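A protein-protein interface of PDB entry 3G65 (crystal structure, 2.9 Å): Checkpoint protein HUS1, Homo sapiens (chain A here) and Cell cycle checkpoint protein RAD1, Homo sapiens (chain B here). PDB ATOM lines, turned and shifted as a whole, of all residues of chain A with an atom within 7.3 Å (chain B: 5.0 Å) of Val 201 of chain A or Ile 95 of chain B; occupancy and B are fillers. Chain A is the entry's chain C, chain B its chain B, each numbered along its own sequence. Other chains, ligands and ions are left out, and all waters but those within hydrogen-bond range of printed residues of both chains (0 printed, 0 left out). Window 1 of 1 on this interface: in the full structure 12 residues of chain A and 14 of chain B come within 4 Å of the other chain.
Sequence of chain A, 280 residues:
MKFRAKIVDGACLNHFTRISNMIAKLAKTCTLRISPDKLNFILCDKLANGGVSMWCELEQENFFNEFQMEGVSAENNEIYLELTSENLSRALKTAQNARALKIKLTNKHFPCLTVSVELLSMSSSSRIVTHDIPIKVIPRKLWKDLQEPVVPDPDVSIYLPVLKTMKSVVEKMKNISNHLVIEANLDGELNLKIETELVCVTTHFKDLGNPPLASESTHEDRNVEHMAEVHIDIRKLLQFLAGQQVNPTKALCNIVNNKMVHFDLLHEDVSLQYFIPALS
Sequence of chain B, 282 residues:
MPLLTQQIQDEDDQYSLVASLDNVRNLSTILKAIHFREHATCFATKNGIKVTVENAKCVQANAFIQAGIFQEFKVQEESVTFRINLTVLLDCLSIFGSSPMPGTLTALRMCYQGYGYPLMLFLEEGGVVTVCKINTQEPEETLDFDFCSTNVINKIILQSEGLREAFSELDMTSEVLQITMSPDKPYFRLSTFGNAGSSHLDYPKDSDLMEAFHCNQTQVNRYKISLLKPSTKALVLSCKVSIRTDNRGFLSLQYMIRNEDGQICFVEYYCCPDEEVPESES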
ATOM      1  N   THR A 165     -21.997 -11.983  -6.198  1.00  0.00           N
ATOM      2  CA  THR A 165     -21.744 -12.694  -4.950  1.00  0.00           C
ATOM      3  C   THR A 165     -22.006 -11.804  -3.738  1.00  0.00           C
ATOM      4  O   THR A 165     -22.621 -12.230  -2.760  1.00  0.00           O
ATOM      5  CB  THR A 165     -20.300 -13.219  -4.884  1.00  0.00           C
ATOM      6  OG1 THR A 165     -20.046 -14.073  -6.008  1.00  0.00           O
ATOM      7  CG2 THR A 165     -20.077 -13.996  -3.594  1.00  0.00           C
ATOM      8  N   MET A 166     -21.530 -10.565  -3.809  1.00  0.00           N
ATOM      9  CA  MET A 166     -21.728  -9.607  -2.730  1.00  0.00           C
ATOM     10  C   MET A 166     -23.215  -9.379  -2.475  1.00  0.00           C
ATOM     11  O   MET A 166     -23.641  -9.189  -1.336  1.00  0.00           O
ATOM     12  CB  MET A 166     -21.040  -8.283  -3.071  1.00  0.00           C
ATOM     13  CG  MET A 166     -21.048  -7.261  -1.947  1.00  0.00           C
ATOM     14  SD  MET A 166     -20.152  -5.756  -2.382  1.00  0.00           S
ATOM     15  CE  MET A 166     -20.347  -4.798  -0.881  1.00  0.00           C
ATOM     16  N   LYS A 167     -23.999  -9.404  -3.549  1.00  0.00           N
ATOM     17  CA  LYS A 167     -25.438  -9.183  -3.467  1.00  0.00           C
ATOM     18  C   LYS A 167     -26.142 -10.335  -2.756  1.00  0.00           C
ATOM     19  O   LYS A 167     -26.983 -10.121  -1.882  1.00  0.00           O
ATOM     20  CB  LYS A 167     -26.021  -8.998  -4.869  1.00  0.00           C
ATOM     21  CG  LYS A 167     -27.519  -8.745  -4.901  1.00  0.00           C
ATOM     22  CD  LYS A 167     -27.992  -8.489  -6.324  1.00  0.00           C
ATOM     23  CE  LYS A 167     -29.482  -8.198  -6.377  1.00  0.00           C
ATOM     24  NZ  LYS A 167     -30.291  -9.365  -5.936  1.00  0.00           N
ATOM     25  N   SER A 168     -25.793 -11.560  -3.136  1.00  0.00           N
ATOM     26  CA  SER A 168     -26.397 -12.746  -2.539  1.00  0.00           C
ATOM     27  C   SER A 168     -26.172 -12.780  -1.032  1.00  0.00           C
ATOM     28  O   SER A 168     -27.058 -13.165  -0.268  1.00  0.00           O
ATOM     29  CB  SER A 168     -25.835 -14.013  -3.182  1.00  0.00           C
ATOM     30  OG  SER A 168     -26.108 -14.044  -4.572  1.00  0.00           O
ATOM     31  N   VAL A 169     -24.979 -12.375  -0.608  1.00  0.00           N
ATOM     32  CA  VAL A 169     -24.641 -12.348   0.808  1.00  0.00           C
ATOM     33  C   VAL A 169     -25.454 -11.290   1.548  1.00  0.00           C
ATOM     34  O   VAL A 169     -26.018 -11.559   2.610  1.00  0.00           O
ATOM     35  CB  VAL A 169     -23.141 -12.078   1.025  1.00  0.00           C
ATOM     36  CG1 VAL A 169     -22.839 -11.936   2.508  1.00  0.00           C
ATOM     37  CG2 VAL A 169     -22.307 -13.190   0.408  1.00  0.00           C
ATOM     38  N   VAL A 170     -25.508 -10.089   0.983  1.00  0.00           N
ATOM     39  CA  VAL A 170     -26.265  -8.994   1.578  1.00  0.00           C
ATOM     40  C   VAL A 170     -27.746  -9.349   1.680  1.00  0.00           C
ATOM     41  O   VAL A 170     -28.409  -9.013   2.662  1.00  0.00           O
ATOM     42  CB  VAL A 170     -26.099  -7.692   0.771  1.00  0.00           C
ATOM     43  CG1 VAL A 170     -27.104  -6.645   1.226  1.00  0.00           C
ATOM     44  CG2 VAL A 170     -24.678  -7.169   0.899  1.00  0.00           C
ATOM     45  N   GLU A 171     -28.261 -10.035   0.664  1.00  0.00           N
ATOM     46  CA  GLU A 171     -29.653 -10.471   0.669  1.00  0.00           C
ATOM     47  C   GLU A 171     -29.976 -11.277   1.922  1.00  0.00           C
ATOM     48  O   GLU A 171     -30.902 -10.946   2.660  1.00  0.00           O
ATOM     49  CB  GLU A 171     -29.963 -11.306  -0.573  1.00  0.00           C
ATOM     50  CG  GLU A 171     -30.166 -10.499  -1.840  1.00  0.00           C
ATOM     51  CD  GLU A 171     -30.578 -11.366  -3.013  1.00  0.00           C
ATOM     52  OE1 GLU A 171     -30.157 -12.542  -3.062  1.00  0.00           O
ATOM     53  OE2 GLU A 171     -31.322 -10.873  -3.886  1.00  0.00           O
ATOM     54  N   LYS A 172     -29.204 -12.332   2.156  1.00  0.00           N
ATOM     55  CA  LYS A 172     -29.443 -13.226   3.284  1.00  0.00           C
ATOM     56  C   LYS A 172     -29.194 -12.540   4.623  1.00  0.00           C
ATOM     57  O   LYS A 172     -29.837 -12.858   5.623  1.00  0.00           O
ATOM     58  CB  LYS A 172     -28.571 -14.476   3.166  1.00  0.00           C
ATOM     59  CG  LYS A 172     -28.796 -15.263   1.886  1.00  0.00           C
ATOM     60  CD  LYS A 172     -30.214 -15.810   1.808  1.00  0.00           C
ATOM     61  CE  LYS A 172     -30.433 -16.589   0.519  1.00  0.00           C
ATOM     62  NZ  LYS A 172     -31.784 -17.210   0.466  1.00  0.00           N
ATOM     63  N   MET A 173     -28.257 -11.599   4.639  1.00  0.00           N
ATOM     64  CA  MET A 173     -27.927 -10.882   5.865  1.00  0.00           C
ATOM     65  C   MET A 173     -29.030  -9.912   6.285  1.00  0.00           C
ATOM     66  O   MET A 173     -29.188  -9.615   7.468  1.00  0.00           O
ATOM     67  CB  MET A 173     -26.597 -10.141   5.716  1.00  0.00           C
ATOM     68  CG  MET A 173     -25.371 -11.040   5.764  1.00  0.00           C
ATOM     69  SD  MET A 173     -23.835 -10.096   5.755  1.00  0.00           S
ATOM     70  CE  MET A 173     -22.634 -11.398   6.023  1.00  0.00           C
ATOM     71  N   ILE A 176     -31.510 -10.983   8.734  1.00  0.00           N
ATOM     72  CA  ILE A 176     -30.984 -11.096  10.089  1.00  0.00           C
ATOM     73  C   ILE A 176     -31.099  -9.770  10.836  1.00  0.00           C
ATOM     74  O   ILE A 176     -31.811  -9.669  11.835  1.00  0.00           O
ATOM     75  CB  ILE A 176     -29.506 -11.531  10.083  1.00  0.00           C
ATOM     76  CG1 ILE A 176     -29.326 -12.807   9.258  1.00  0.00           C
ATOM     77  CG2 ILE A 176     -29.003 -11.733  11.505  1.00  0.00           C
ATOM     78  CD1 ILE A 176     -29.921 -14.040   9.898  1.00  0.00           C
ATOM     79  N   VAL A 181     -21.788  -3.871   9.100  1.00  0.00           N
ATOM     80  CA  VAL A 181     -20.454  -3.298   9.217  1.00  0.00           C
ATOM     81  C   VAL A 181     -19.560  -3.779   8.082  1.00  0.00           C
ATOM     82  O   VAL A 181     -19.257  -4.968   7.980  1.00  0.00           O
ATOM     83  CB  VAL A 181     -19.799  -3.662  10.560  1.00  0.00           C
ATOM     84  CG1 VAL A 181     -18.402  -3.068  10.644  1.00  0.00           C
ATOM     85  CG2 VAL A 181     -20.659  -3.182  11.718  1.00  0.00           C
ATOM     86  N   LEU A 192     -17.780  -8.355   5.577  1.00  0.00           N
ATOM     87  CA  LEU A 192     -19.157  -7.963   5.846  1.00  0.00           C
ATOM     88  C   LEU A 192     -19.609  -8.561   7.174  1.00  0.00           C
ATOM     89  O   LEU A 192     -19.726  -9.778   7.306  1.00  0.00           O
ATOM     90  CB  LEU A 192     -20.079  -8.419   4.714  1.00  0.00           C
ATOM     91  CG  LEU A 192     -19.792  -7.823   3.332  1.00  0.00           C
ATOM     92  CD1 LEU A 192     -20.721  -8.417   2.284  1.00  0.00           C
ATOM     93  CD2 LEU A 192     -19.913  -6.306   3.363  1.00  0.00           C
ATOM     94  N   LYS A 193     -19.859  -7.702   8.156  1.00  0.00           N
ATOM     95  CA  LYS A 193     -20.193  -8.162   9.499  1.00  0.00           C
ATOM     96  C   LYS A 193     -21.574  -7.713   9.965  1.00  0.00           C
ATOM     97  O   LYS A 193     -21.896  -6.527   9.942  1.00  0.00           O
ATOM     98  CB  LYS A 193     -19.133  -7.694  10.499  1.00  0.00           C
ATOM     99  CG  LYS A 193     -17.760  -8.309  10.288  1.00  0.00           C
ATOM    100  CD  LYS A 193     -16.826  -7.971  11.440  1.00  0.00           C
ATOM    101  CE  LYS A 193     -15.493  -8.686  11.299  1.00  0.00           C
ATOM    102  NZ  LYS A 193     -14.592  -8.412  12.453  1.00  0.00           N
ATOM    103  N   ILE A 194     -22.384  -8.676  10.392  1.00  0.00           N
ATOM    104  CA  ILE A 194     -23.659  -8.382  11.031  1.00  0.00           C
ATOM    105  C   ILE A 194     -23.690  -9.057  12.396  1.00  0.00           C
ATOM    106  O   ILE A 194     -23.254 -10.199  12.540  1.00  0.00           O
ATOM    107  CB  ILE A 194     -24.855  -8.866  10.188  1.00  0.00           C
ATOM    108  CG1 ILE A 194     -24.850 -10.391  10.076  1.00  0.00           C
ATOM    109  CG2 ILE A 194     -24.831  -8.222   8.809  1.00  0.00           C
ATOM    110  CD1 ILE A 194     -26.066 -10.956   9.375  1.00  0.00           C
ATOM    111  N   GLU A 195     -24.195  -8.349  13.401  1.00  0.00           N
ATOM    112  CA  GLU A 195     -24.200  -8.876  14.760  1.00  0.00           C
ATOM    113  C   GLU A 195     -25.512  -8.608  15.488  1.00  0.00           C
ATOM    114  O   GLU A 195     -25.908  -7.458  15.681  1.00  0.00           O
ATOM    115  CB  GLU A 195     -23.033  -8.299  15.566  1.00  0.00           C
ATOM    116  CG  GLU A 195     -21.661  -8.735  15.080  1.00  0.00           C
ATOM    117  CD  GLU A 195     -20.546  -8.284  16.004  1.00  0.00           C
ATOM    118  OE1 GLU A 195     -20.851  -7.694  17.062  1.00  0.00           O
ATOM    119  OE2 GLU A 195     -19.366  -8.521  15.673  1.00  0.00           O
ATOM    120  N   THR A 196     -26.180  -9.683  15.891  1.00  0.00           N
ATOM    121  CA  THR A 196     -27.369  -9.580  16.725  1.00  0.00           C
ATOM    122  C   THR A 196     -27.124 -10.320  18.035  1.00  0.00           C
ATOM    123  O   THR A 196     -26.131 -11.033  18.174  1.00  0.00           O
ATOM    124  CB  THR A 196     -28.608 -10.168  16.027  1.00  0.00           C
ATOM    125  OG1 THR A 196     -28.431 -11.576  15.835  1.00  0.00           O
ATOM    126  CG2 THR A 196     -28.827  -9.498  14.680  1.00  0.00           C
ATOM    127  N   VAL A 199     -27.392 -14.117  16.674  1.00  0.00           N
ATOM    128  CA  VAL A 199     -26.690 -14.603  15.490  1.00  0.00           C
ATOM    129  C   VAL A 199     -25.634 -13.614  15.007  1.00  0.00           C
ATOM    130  O   VAL A 199     -25.879 -12.410  14.943  1.00  0.00           O
ATOM    131  CB  VAL A 199     -27.670 -14.884  14.334  1.00  0.00           C
ATOM    132  CG1 VAL A 199     -26.921 -15.426  13.124  1.00  0.00           C
ATOM    133  CG2 VAL A 199     -28.752 -15.854  14.776  1.00  0.00           C
ATOM    134  N   CYS A 200     -24.458 -14.133  14.668  1.00  0.00           N
ATOM    135  CA  CYS A 200     -23.382 -13.314  14.122  1.00  0.00           C
ATOM    136  C   CYS A 200     -22.856 -13.925  12.828  1.00  0.00           C
ATOM    137  O   CYS A 200     -22.481 -15.097  12.794  1.00  0.00           O
ATOM    138  CB  CYS A 200     -22.247 -13.166  15.138  1.00  0.00           C
ATOM    139  SG  CYS A 200     -22.714 -12.323  16.668  1.00  0.00           S
ATOM    140  N   VAL A 201     -22.837 -13.130  11.764  1.00  0.00           N
ATOM    141  CA  VAL A 201     -22.368 -13.608  10.468  1.00  0.00           C
ATOM    142  C   VAL A 201     -21.305 -12.684   9.887  1.00  0.00           C
ATOM    143  O   VAL A 201     -21.503 -11.472   9.799  1.00  0.00           O
ATOM    144  CB  VAL A 201     -23.525 -13.742   9.459  1.00  0.00           C
ATOM    145  CG1 VAL A 201     -23.013 -14.312   8.147  1.00  0.00           C
ATOM    146  CG2 VAL A 201     -24.631 -14.616  10.029  1.00  0.00           C
ATOM    147  N   THR A 202     -20.178 -13.263   9.489  1.00  0.00           N
ATOM    148  CA  THR A 202     -19.079 -12.491   8.925  1.00  0.00           C
ATOM    149  C   THR A 202     -18.543 -13.133   7.650  1.00  0.00           C
ATOM    150  O   THR A 202     -18.117 -14.286   7.658  1.00  0.00           O
ATOM    151  CB  THR A 202     -17.926 -12.333   9.935  1.00  0.00           C
ATOM    152  OG1 THR A 202     -18.384 -11.593  11.073  1.00  0.00           O
ATOM    153  CG2 THR A 202     -16.759 -11.597   9.299  1.00  0.00           C
ATOM    154  N   THR A 203     -18.569 -12.378   6.556  1.00  0.00           N
ATOM    155  CA  THR A 203     -18.058 -12.859   5.278  1.00  0.00           C
ATOM    156  C   THR A 203     -16.683 -12.264   4.992  1.00  0.00           C
ATOM    157  O   THR A 203     -16.458 -11.073   5.202  1.00  0.00           O
ATOM    158  CB  THR A 203     -19.012 -12.510   4.125  1.00  0.00           C
ATOM    159  OG1 THR A 203     -20.296 -13.093   4.376  1.00  0.00           O
ATOM    160  CG2 THR A 203     -18.472 -13.039   2.805  1.00  0.00           C
ATOM    161  N   HIS A 204     -15.769 -13.100   4.510  1.00  0.00           N
ATOM    162  CA  HIS A 204     -14.390 -12.679   4.287  1.00  0.00           C
ATOM    163  C   HIS A 204     -13.987 -12.763   2.817  1.00  0.00           C
ATOM    164  O   HIS A 204     -13.903 -13.851   2.247  1.00  0.00           O
ATOM    165  CB  HIS A 204     -13.431 -13.520   5.136  1.00  0.00           C
ATOM    166  CG  HIS A 204     -13.743 -13.503   6.601  1.00  0.00           C
ATOM    167  ND1 HIS A 204     -13.186 -12.591   7.471  1.00  0.00           N
ATOM    168  CD2 HIS A 204     -14.550 -14.292   7.350  1.00  0.00           C
ATOM    169  CE1 HIS A 204     -13.638 -12.816   8.692  1.00  0.00           C
ATOM    170  NE2 HIS A 204     -14.468 -13.842   8.646  1.00  0.00           N
ATOM    171  N   ASP B  91     -30.833 -19.628   6.042  1.00  0.00           N
ATOM    172  CA  ASP B  91     -30.331 -18.395   5.447  1.00  0.00           C
ATOM    173  C   ASP B  91     -28.808 -18.392   5.417  1.00  0.00           C
ATOM    174  O   ASP B  91     -28.198 -17.920   4.457  1.00  0.00           O
ATOM    175  CB  ASP B  91     -30.844 -17.174   6.211  1.00  0.00           C
ATOM    176  CG  ASP B  91     -32.277 -16.827   5.862  1.00  0.00           C
ATOM    177  OD1 ASP B  91     -32.822 -17.426   4.911  1.00  0.00           O
ATOM    178  OD2 ASP B  91     -32.857 -15.951   6.537  1.00  0.00           O
ATOM    179  N   CYS B  92     -28.201 -18.924   6.471  1.00  0.00           N
ATOM    180  CA  CYS B  92     -26.748 -18.979   6.570  1.00  0.00           C
ATOM    181  C   CYS B  92     -26.153 -19.956   5.561  1.00  0.00           C
ATOM    182  O   CYS B  92     -25.157 -19.652   4.909  1.00  0.00           O
ATOM    183  CB  CYS B  92     -26.314 -19.348   7.990  1.00  0.00           C
ATOM    184  SG  CYS B  92     -26.637 -18.067   9.230  1.00  0.00           S
ATOM    185  N   LEU B  93     -26.771 -21.126   5.434  1.00  0.00           N
ATOM    186  CA  LEU B  93     -26.293 -22.144   4.506  1.00  0.00           C
ATOM    187  C   LEU B  93     -26.306 -21.641   3.066  1.00  0.00           C
ATOM    188  O   LEU B  93     -25.310 -21.745   2.354  1.00  0.00           O
ATOM    189  CB  LEU B  93     -27.132 -23.417   4.629  1.00  0.00           C
ATOM    190  CG  LEU B  93     -27.111 -24.120   5.990  1.00  0.00           C
ATOM    191  CD1 LEU B  93     -28.034 -25.329   5.987  1.00  0.00           C
ATOM    192  CD2 LEU B  93     -25.694 -24.529   6.358  1.00  0.00           C
ATOM    193  N   SER B  94     -27.438 -21.090   2.643  1.00  0.00           N
ATOM    194  CA  SER B  94     -27.575 -20.578   1.287  1.00  0.00           C
ATOM    195  C   SER B  94     -27.216 -19.097   1.220  1.00  0.00           C
ATOM    196  O   SER B  94     -27.875 -18.320   0.531  1.00  0.00           O
ATOM    197  CB  SER B  94     -29.001 -20.799   0.776  1.00  0.00           C
ATOM    198  OG  SER B  94     -29.947 -20.192   1.637  1.00  0.00           O
ATOM    199  N   ILE B  95     -26.163 -18.712   1.935  1.00  0.00           N
ATOM    200  CA  ILE B  95     -25.747 -17.313   1.991  1.00  0.00           C
ATOM    201  C   ILE B  95     -25.082 -16.854   0.693  1.00  0.00           C
ATOM    202  O   ILE B  95     -25.219 -15.698   0.295  1.00  0.00           O
ATOM    203  CB  ILE B  95     -24.803 -17.044   3.185  1.00  0.00           C
ATOM    204  CG1 ILE B  95     -24.628 -15.540   3.402  1.00  0.00           C
ATOM    205  CG2 ILE B  95     -23.457 -17.723   2.972  1.00  0.00           C
ATOM    206  CD1 ILE B  95     -23.858 -15.188   4.653  1.00  0.00           C
ATOM    207  N   PHE B  96     -24.366 -17.762   0.036  1.00  0.00           N
ATOM    208  CA  PHE B  96     -23.709 -17.447  -1.228  1.00  0.00           C
ATOM    209  C   PHE B  96     -24.676 -17.563  -2.402  1.00  0.00           C
ATOM    210  O   PHE B  96     -24.284 -17.930  -3.508  1.00  0.00           O
ATOM    211  CB  PHE B  96     -22.503 -18.361  -1.454  1.00  0.00           C
ATOM    212  CG  PHE B  96     -21.381 -18.142  -0.479  1.00  0.00           C
ATOM    213  CD1 PHE B  96     -20.581 -17.013  -0.561  1.00  0.00           C
ATOM    214  CD2 PHE B  96     -21.117 -19.070   0.515  1.00  0.00           C
ATOM    215  CE1 PHE B  96     -19.549 -16.809   0.333  1.00  0.00           C
ATOM    216  CE2 PHE B  96     -20.086 -18.874   1.412  1.00  0.00           C
ATOM    217  CZ  PHE B  96     -19.301 -17.742   1.321  1.00  0.00           C
ATOM    218  N   GLY B  97     -25.942 -17.242  -2.155  1.00  0.00           N
ATOM    219  CA  GLY B  97     -26.962 -17.339  -3.180  1.00  0.00           C
ATOM    220  C   GLY B  97     -27.434 -18.766  -3.371  1.00  0.00           C
ATOM    221  O   GLY B  97     -26.714 -19.718  -3.066  1.00  0.00           O
ATOM    222  N   LEU B 123     -18.598 -21.805   5.898  1.00  0.00           N
ATOM    223  CA  LEU B 123     -18.902 -21.983   4.484  1.00  0.00           C
ATOM    224  C   LEU B 123     -17.886 -21.267   3.603  1.00  0.00           C
ATOM    225  O   LEU B 123     -17.292 -20.267   4.009  1.00  0.00           O
ATOM    226  CB  LEU B 123     -20.311 -21.475   4.179  1.00  0.00           C
ATOM    227  CG  LEU B 123     -21.432 -22.111   5.001  1.00  0.00           C
ATOM    228  CD1 LEU B 123     -22.700 -21.281   4.929  1.00  0.00           C
ATOM    229  CD2 LEU B 123     -21.689 -23.532   4.533  1.00  0.00           C
ATOM    230  N   THR B 130     -17.246 -17.598   4.903  1.00  0.00           N
ATOM    231  CA  THR B 130     -18.150 -16.950   5.845  1.00  0.00           C
ATOM    232  C   THR B 130     -18.278 -17.774   7.123  1.00  0.00           C
ATOM    233  O   THR B 130     -18.299 -19.005   7.080  1.00  0.00           O
ATOM    234  CB  THR B 130     -19.547 -16.733   5.234  1.00  0.00           C
ATOM    235  OG1 THR B 130     -20.413 -16.140   6.209  1.00  0.00           O
ATOM    236  CG2 THR B 130     -20.142 -18.055   4.777  1.00  0.00           C
ATOM    237  N   VAL B 131     -18.360 -17.087   8.258  1.00  0.00           N
ATOM    238  CA  VAL B 131     -18.463 -17.747   9.553  1.00  0.00           C
ATOM    239  C   VAL B 131     -19.717 -17.296  10.288  1.00  0.00           C
ATOM    240  O   VAL B 131     -19.915 -16.105  10.527  1.00  0.00           O
ATOM    241  CB  VAL B 131     -17.234 -17.451  10.431  1.00  0.00           C
ATOM    242  CG1 VAL B 131     -17.356 -18.155  11.774  1.00  0.00           C
ATOM    243  CG2 VAL B 131     -15.958 -17.868   9.715  1.00  0.00           C
ATOM    244  N   CYS B 132     -20.563 -18.255  10.648  1.00  0.00           N
ATOM    245  CA  CYS B 132     -21.816 -17.951  11.330  1.00  0.00           C
ATOM    246  C   CYS B 132     -21.796 -18.421  12.782  1.00  0.00           C
ATOM    247  O   CYS B 132     -21.149 -19.414  13.119  1.00  0.00           O
ATOM    248  CB  CYS B 132     -22.995 -18.578  10.582  1.00  0.00           C
ATOM    249  SG  CYS B 132     -23.134 -18.064   8.852  1.00  0.00           S
ATOM    250  N   LYS B 133     -22.508 -17.697  13.639  1.00  0.00           N
ATOM    251  CA  LYS B 133     -22.568 -18.020  15.059  1.00  0.00           C
ATOM    252  C   LYS B 133     -24.010 -17.978  15.553  1.00  0.00           C
ATOM    253  O   LYS B 133     -24.486 -16.942  16.015  1.00  0.00           O
ATOM    254  CB  LYS B 133     -21.712 -17.038  15.860  1.00  0.00           C
ATOM    255  CG  LYS B 133     -20.353 -16.757  15.240  1.00  0.00           C
ATOM    256  CD  LYS B 133     -19.607 -15.673  15.999  1.00  0.00           C
ATOM    257  CE  LYS B 133     -18.383 -15.208  15.228  1.00  0.00           C
ATOM    258  NZ  LYS B 133     -17.476 -16.340  14.888  1.00  0.00           N
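N of Val 131 of chain B lies within hydrogen-bond range of O of Thr 202 of chain A (2.9 Å). The backbone NH (N) of Lys 133 of chain B sits at hydrogen-bond distance from the backbone carbonyl oxygen (O) of Cys 200 of chain A, 2.7 Å away. The backbone carbonyl oxygen (O) of Thr 202 of chain A sits close to the side-chain hydroxyl (OG1) of Thr 130 of chain B (3.3 Å). The backbone carbonyl oxygen of Ser 168 of chain A lies close to the backbone carbonyl oxygen of Ile 95 of chain B, 3.2 Å away. O of Ile 95 of chain B lies close to N of Val 169 of chain A (3.5 Å).
The backbone carbonyl oxygen (O) of Val 199 of chain A is in hydrogen-bond range of the side-chain hydroxyl (OG1) of Thr 196 of chain A. The backbone carbonyl oxygen (O) of Leu 192 of chain A is in hydrogen-bond range of the backbone NH (N) of Thr 203 of chain A, 2.9 Å away. O of Val 201 of chain A lies within hydrogen-bond range of N of Ile 194 of chain A, 3.0 Å away. SG of Cys 92 of chain B lies within hydrogen-bond range of SG of Cys 132 of chain B (3.5 Å). The backbone NH of Thr 130 of chain B lies within hydrogen-bond range of the backbone carbonyl oxygen of Leu 123 of chain B.
Among the printed residues, merely in contact across the chains: Ser 168 of chain A with Phe 96 of chain B, Ser 168 of chain A with Gly 97 of chain B, Lys 172 of chain A with Asp 91 of chain B, Lys 172 of chain A with Ser 94 of chain B, Lys 172 of chain A with Ile 95 of chain B, Val 199 of chain A with Lys 133 of chain B, Cys 200 of chain A with Val 131 of chain B, Cys 200 of chain A with Cys 132 of chain B, Val 201 of chain A with Ile 95 of chain B, Val 201 of chain A with Thr 130 of chain B, Val 201 of chain A with Val 131 of chain B, Val 201 of chain A with Cys 132 of chain B and Thr 203 of chain A with Thr 130 of chain B.
Printed residues of chain B within 4 Å of Val 201 of chain A: Ile 95, Thr 130, Val 131 and Cys 132. Of the printed residues of chain A, Ile 95 of chain B touches Ser 168, Val 169, Lys 172 and Val 201. Of the printed residues of chain A, Lys 133 of chain B touches Val 199 (3.3 Å) and Cys 200 (2.7 Å). Of the printed residues of chain A, Phe 96 of chain B touches Ser 168. Of the printed residues of chain B, Lys 172 of chain A touches Asp 91, Ser 94 and Ile 95. Printed residues of chain A within 4 Å of Cys 132 of chain B: Cys 200 (3.3 Å) and Val 201 (3.8 Å). Met 166 of chain A touches none of the printed residues of chain B. Val 170 of chain A touches none of the printed residues of chain B. The nearest residue of chain B that does not touch Val 201 of chain A is Cys 92 of chain B (4.1 Å). The nearest residue of chain A that does not touch Ile 95 of chain B is Thr 203 of chain A (4.1 Å).
Of the 12 printed residues of chain B, 9 touch a printed residue of chain A. Hydrophobic or aromatic side chains of chain B within 4 Å of the printed part of chain A: Ile 95. Along chain B the printed residues that touch a printed residue of chain A span positions 91 to 133. Of the 22 printed residues of chain A, 8 touch a printed residue of chain B. Hydrophobic or aromatic side chains of chain A that line the printed part of chain B: Val 169 and Val 201. Among the printed residues, 18 pairs touch across the chains. Among the printed residues, no Asp or Glu carboxylate lies within 4 Å of a Lys or Arg side-chain nitrogen of the other chain.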
